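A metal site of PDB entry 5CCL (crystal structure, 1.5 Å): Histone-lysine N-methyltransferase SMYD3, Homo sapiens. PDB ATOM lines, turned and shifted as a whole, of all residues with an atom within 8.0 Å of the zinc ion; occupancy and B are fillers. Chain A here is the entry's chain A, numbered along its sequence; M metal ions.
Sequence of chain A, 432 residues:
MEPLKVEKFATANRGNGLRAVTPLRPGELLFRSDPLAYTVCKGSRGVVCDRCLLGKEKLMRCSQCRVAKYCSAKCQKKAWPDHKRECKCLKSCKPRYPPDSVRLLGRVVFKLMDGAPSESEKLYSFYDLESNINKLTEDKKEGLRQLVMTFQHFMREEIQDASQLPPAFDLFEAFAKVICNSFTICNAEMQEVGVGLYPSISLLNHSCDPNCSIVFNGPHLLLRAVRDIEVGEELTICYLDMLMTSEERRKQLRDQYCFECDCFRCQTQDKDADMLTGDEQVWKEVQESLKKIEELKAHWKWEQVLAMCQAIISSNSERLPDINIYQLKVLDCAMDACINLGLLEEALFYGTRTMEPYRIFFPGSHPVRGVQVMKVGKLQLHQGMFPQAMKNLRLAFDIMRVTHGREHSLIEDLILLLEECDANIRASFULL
The zinc ion is bound by SG of Cys 52 (2.3 Å), SG of Cys 71 (2.3 Å), SG of Cys 75 (2.3 Å) and SG of Cys 49 (2.3 Å).
The zinc ion has four donor atoms within binding distance.
The backbone NH (N) of Leu 54 lies close to the side-chain sulfur (SG) of Cys 52, 3.7 Å away.
OG of Ser 72 sits close to SG of Cys 71.
The side-chain hydroxyl of Ser 72 lies within hydrogen-bond range of the backbone NH of Cys 75.
SG of Cys 75 lies close to NE of Arg 51 (3.1 Å).
The backbone NH (N) of Arg 51 lies close to the side-chain sulfur (SG) of Cys 49, at 3.5 Å.
The backbone carbonyl oxygen of Leu 54 is in hydrogen-bond range of the backbone NH of Cys 49 (2.9 Å).
Four residues have an atom within 4 Å of the zinc ion: Cys 49, Cys 52, Cys 71 and Cys 75.
Along chain A the residues within 4 Å of the zinc ion span positions 49 to 75.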
ATOM      1  N   VAL A  48     -15.020 -28.479 -29.354  1.00  0.00           N
ATOM      2  CA  VAL A  48     -14.193 -28.419 -28.164  1.00  0.00           C
ATOM      3  C   VAL A  48     -12.726 -28.317 -28.583  1.00  0.00           C
ATOM      4  O   VAL A  48     -12.344 -28.754 -29.676  1.00  0.00           O
ATOM      5  CB  VAL A  48     -14.379 -29.583 -27.203  1.00  0.00           C
ATOM      6  CG1 VAL A  48     -15.843 -29.828 -26.882  1.00  0.00           C
ATOM      7  CG2 VAL A  48     -13.779 -30.842 -27.739  1.00  0.00           C
ATOM      8  N   CYS A  49     -11.925 -27.753 -27.710  1.00  0.00           N
ATOM      9  CA  CYS A  49     -10.489 -27.643 -27.941  1.00  0.00           C
ATOM     10  C   CYS A  49      -9.858 -28.993 -27.982  1.00  0.00           C
ATOM     11  O   CYS A  49     -10.053 -29.830 -27.103  1.00  0.00           O
ATOM     12  CB  CYS A  49      -9.901 -26.827 -26.814  1.00  0.00           C
ATOM     13  SG  CYS A  49      -8.108 -26.608 -26.819  1.00  0.00           S
ATOM     14  N   ASP A  50      -9.008 -29.206 -28.979  1.00  0.00           N
ATOM     15  CA  ASP A  50      -8.313 -30.472 -29.143  1.00  0.00           C
ATOM     16  C   ASP A  50      -7.439 -30.830 -27.960  1.00  0.00           C
ATOM     17  O   ASP A  50      -7.199 -32.008 -27.749  1.00  0.00           O
ATOM     18  CB  ASP A  50      -7.348 -30.377 -30.343  1.00  0.00           C
ATOM     19  CG  ASP A  50      -7.881 -30.878 -31.637  1.00  0.00           C
ATOM     20  OD1 ASP A  50      -8.921 -30.399 -32.150  1.00  0.00           O
ATOM     21  OD2 ASP A  50      -7.101 -31.682 -32.197  1.00  0.00           O
ATOM     22  N   ARG A  51      -6.913 -29.836 -27.210  1.00  0.00           N
ATOM     23  CA  ARG A  51      -6.058 -30.150 -26.082  1.00  0.00           C
ATOM     24  C   ARG A  51      -6.862 -30.279 -24.791  1.00  0.00           C
ATOM     25  O   ARG A  51      -6.878 -31.342 -24.171  1.00  0.00           O
ATOM     26  CB  ARG A  51      -4.931 -29.152 -25.888  1.00  0.00           C
ATOM     27  CG  ARG A  51      -3.885 -29.735 -24.935  1.00  0.00           C
ATOM     28  CD  ARG A  51      -3.016 -28.671 -24.322  1.00  0.00           C
ATOM     29  NE  ARG A  51      -3.780 -27.856 -23.397  1.00  0.00           N
ATOM     30  CZ  ARG A  51      -3.486 -27.709 -22.113  1.00  0.00           C
ATOM     31  NH1 ARG A  51      -4.250 -26.946 -21.376  1.00  0.00           N
ATOM     32  NH2 ARG A  51      -2.430 -28.342 -21.581  1.00  0.00           N
ATOM     33  N   CYS A  52      -7.555 -29.222 -24.399  1.00  0.00           N
ATOM     34  CA  CYS A  52      -8.119 -29.212 -23.045  1.00  0.00           C
ATOM     35  C   CYS A  52      -9.517 -29.821 -23.027  1.00  0.00           C
ATOM     36  O   CYS A  52     -10.076 -30.033 -21.939  1.00  0.00           O
ATOM     37  CB  CYS A  52      -8.098 -27.801 -22.441  1.00  0.00           C
ATOM     38  SG  CYS A  52      -9.241 -26.629 -23.253  1.00  0.00           S
ATOM     39  N   LEU A  53     -10.116 -30.087 -24.192  1.00  0.00           N
ATOM     40  CA  LEU A  53     -11.443 -30.738 -24.286  1.00  0.00           C
ATOM     41  C   LEU A  53     -12.560 -29.897 -23.676  1.00  0.00           C
ATOM     42  O   LEU A  53     -13.607 -30.445 -23.317  1.00  0.00           O
ATOM     43  CB  LEU A  53     -11.408 -32.161 -23.748  1.00  0.00           C
ATOM     44  CG  LEU A  53     -10.342 -33.055 -24.362  1.00  0.00           C
ATOM     45  CD1 LEU A  53     -10.382 -34.429 -23.707  1.00  0.00           C
ATOM     46  CD2 LEU A  53     -10.596 -33.209 -25.829  1.00  0.00           C
ATOM     47  N   LEU A  54     -12.368 -28.557 -23.659  1.00  0.00           N
ATOM     48  CA  LEU A  54     -13.424 -27.617 -23.265  1.00  0.00           C
ATOM     49  C   LEU A  54     -14.110 -26.973 -24.458  1.00  0.00           C
ATOM     50  O   LEU A  54     -13.476 -26.650 -25.458  1.00  0.00           O
ATOM     51  CB  LEU A  54     -12.863 -26.517 -22.376  1.00  0.00           C
ATOM     52  CG  LEU A  54     -12.179 -26.969 -21.095  1.00  0.00           C
ATOM     53  CD1 LEU A  54     -11.721 -25.771 -20.324  1.00  0.00           C
ATOM     54  CD2 LEU A  54     -13.110 -27.785 -20.198  1.00  0.00           C
ATOM     55  N   GLY A  55     -15.418 -26.767 -24.340  1.00  0.00           N
ATOM     56  CA  GLY A  55     -16.182 -26.082 -25.351  1.00  0.00           C
ATOM     57  C   GLY A  55     -16.019 -24.576 -25.196  1.00  0.00           C
ATOM     58  O   GLY A  55     -16.103 -24.039 -24.111  1.00  0.00           O
ATOM     59  N   LYS A  56     -15.728 -23.895 -26.290  1.00  0.00           N
ATOM     60  CA  LYS A  56     -15.652 -22.440 -26.275  1.00  0.00           C
ATOM     61  C   LYS A  56     -16.365 -21.863 -27.490  1.00  0.00           C
ATOM     62  O   LYS A  56     -16.562 -22.544 -28.513  1.00  0.00           O
ATOM     63  CB  LYS A  56     -14.200 -21.944 -26.246  1.00  0.00           C
ATOM     64  CG  LYS A  56     -13.728 -21.441 -24.890  1.00  0.00           C
ATOM     65  CD  LYS A  56     -13.061 -22.547 -24.096  1.00  0.00           C
ATOM     66  CE  LYS A  56     -12.794 -22.090 -22.663  1.00  0.00           C
ATOM     67  NZ  LYS A  56     -11.426 -22.468 -22.246  1.00  0.00           N
ATOM     68  N   LEU A  59     -12.883 -21.127 -31.234  1.00  0.00           N
ATOM     69  CA  LEU A  59     -11.679 -21.932 -31.389  1.00  0.00           C
ATOM     70  C   LEU A  59     -10.906 -21.421 -32.596  1.00  0.00           C
ATOM     71  O   LEU A  59     -11.496 -20.791 -33.516  1.00  0.00           O
ATOM     72  CB  LEU A  59     -12.032 -23.418 -31.602  1.00  0.00           C
ATOM     73  CG  LEU A  59     -12.804 -24.032 -30.438  1.00  0.00           C
ATOM     74  CD1 LEU A  59     -13.154 -25.474 -30.801  1.00  0.00           C
ATOM     75  CD2 LEU A  59     -11.999 -24.036 -29.143  1.00  0.00           C
ATOM     76  N   LYS A  69      -8.172 -27.764 -33.680  1.00  0.00           N
ATOM     77  CA  LYS A  69      -8.688 -26.492 -33.210  1.00  0.00           C
ATOM     78  C   LYS A  69      -8.372 -26.327 -31.731  1.00  0.00           C
ATOM     79  O   LYS A  69      -8.446 -27.310 -30.969  1.00  0.00           O
ATOM     80  CB  LYS A  69     -10.189 -26.411 -33.450  1.00  0.00           C
ATOM     81  CG  LYS A  69     -10.550 -26.230 -34.934  1.00  0.00           C
ATOM     82  CD  LYS A  69     -11.983 -25.803 -35.152  1.00  0.00           C
ATOM     83  CE  LYS A  69     -12.290 -25.628 -36.645  1.00  0.00           C
ATOM     84  NZ  LYS A  69     -13.327 -26.540 -37.219  1.00  0.00           N
ATOM     85  N   TYR A  70      -7.983 -25.103 -31.358  1.00  0.00           N
ATOM     86  CA  TYR A  70      -7.558 -24.766 -30.013  1.00  0.00           C
ATOM     87  C   TYR A  70      -8.265 -23.560 -29.447  1.00  0.00           C
ATOM     88  O   TYR A  70      -8.594 -22.617 -30.194  1.00  0.00           O
ATOM     89  CB  TYR A  70      -6.029 -24.521 -29.972  1.00  0.00           C
ATOM     90  CG  TYR A  70      -5.221 -25.704 -30.477  1.00  0.00           C
ATOM     91  CD1 TYR A  70      -5.118 -26.868 -29.706  1.00  0.00           C
ATOM     92  CD2 TYR A  70      -4.600 -25.686 -31.716  1.00  0.00           C
ATOM     93  CE1 TYR A  70      -4.429 -27.976 -30.180  1.00  0.00           C
ATOM     94  CE2 TYR A  70      -3.914 -26.785 -32.167  1.00  0.00           C
ATOM     95  CZ  TYR A  70      -3.810 -27.901 -31.406  1.00  0.00           C
ATOM     96  OH  TYR A  70      -3.119 -28.987 -31.888  1.00  0.00           O
ATOM     97  N   CYS A  71      -8.467 -23.556 -28.131  1.00  0.00           N
ATOM     98  CA  CYS A  71      -9.112 -22.422 -27.459  1.00  0.00           C
ATOM     99  C   CYS A  71      -8.179 -21.258 -27.283  1.00  0.00           C
ATOM    100  O   CYS A  71      -8.643 -20.187 -26.944  1.00  0.00           O
ATOM    101  CB  CYS A  71      -9.669 -22.845 -26.102  1.00  0.00           C
ATOM    102  SG  CYS A  71      -8.469 -23.268 -24.867  1.00  0.00           S
ATOM    103  N   SER A  72      -6.867 -21.469 -27.447  1.00  0.00           N
ATOM    104  CA  SER A  72      -5.882 -20.530 -26.947  1.00  0.00           C
ATOM    105  C   SER A  72      -4.487 -20.871 -27.443  1.00  0.00           C
ATOM    106  O   SER A  72      -4.203 -21.996 -27.804  1.00  0.00           O
ATOM    107  CB  SER A  72      -5.845 -20.586 -25.393  1.00  0.00           C
ATOM    108  OG  SER A  72      -5.469 -21.883 -24.920  1.00  0.00           O
ATOM    109  N   ALA A  73      -3.611 -19.890 -27.374  1.00  0.00           N
ATOM    110  CA  ALA A  73      -2.229 -20.113 -27.653  1.00  0.00           C
ATOM    111  C   ALA A  73      -1.663 -21.102 -26.670  1.00  0.00           C
ATOM    112  O   ALA A  73      -0.874 -21.927 -27.066  1.00  0.00           O
ATOM    113  CB  ALA A  73      -1.469 -18.818 -27.581  1.00  0.00           C
ATOM    114  N   LYS A  74      -2.084 -21.043 -25.406  1.00  0.00           N
ATOM    115  CA  LYS A  74      -1.584 -21.989 -24.399  1.00  0.00           C
ATOM    116  C   LYS A  74      -1.837 -23.409 -24.886  1.00  0.00           C
ATOM    117  O   LYS A  74      -0.974 -24.280 -24.871  1.00  0.00           O
ATOM    118  CB  LYS A  74      -2.286 -21.724 -23.052  1.00  0.00           C
ATOM    119  CG  LYS A  74      -1.996 -22.729 -21.937  1.00  0.00           C
ATOM    120  CD  LYS A  74      -2.666 -22.322 -20.611  1.00  0.00           C
ATOM    121  CE  LYS A  74      -2.554 -23.466 -19.604  1.00  0.00           C
ATOM    122  NZ  LYS A  74      -3.327 -23.255 -18.345  1.00  0.00           N
ATOM    123  N   CYS A  75      -3.067 -23.641 -25.293  1.00  0.00           N
ATOM    124  CA  CYS A  75      -3.394 -25.004 -25.745  1.00  0.00           C
ATOM    125  C   CYS A  75      -2.692 -25.427 -27.026  1.00  0.00           C
ATOM    126  O   CYS A  75      -2.254 -26.560 -27.153  1.00  0.00           O
ATOM    127  CB  CYS A  75      -4.890 -25.196 -25.851  1.00  0.00           C
ATOM    128  SG  CYS A  75      -5.648 -25.483 -24.200  1.00  0.00           S
ATOM    129  N   GLN A  76      -2.594 -24.526 -28.009  1.00  0.00           N
ATOM    130  CA  GLN A  76      -1.885 -24.894 -29.231  1.00  0.00           C
ATOM    131  C   GLN A  76      -0.433 -25.304 -28.911  1.00  0.00           C
ATOM    132  O   GLN A  76       0.087 -26.242 -29.463  1.00  0.00           O
ATOM    133  CB  GLN A  76      -1.832 -23.682 -30.134  1.00  0.00           C
ATOM    134  CG  GLN A  76      -1.293 -23.985 -31.494  1.00  0.00           C
ATOM    135  CD  GLN A  76       0.193 -23.800 -31.626  1.00  0.00           C
ATOM    136  OE1 GLN A  76       0.856 -24.510 -32.418  1.00  0.00           O
ATOM    137  NE2 GLN A  76       0.736 -22.850 -30.896  1.00  0.00           N
HETATM  138 ZN    ZN M   1      -7.900 -25.512 -24.771  1.00  0.00          ZN
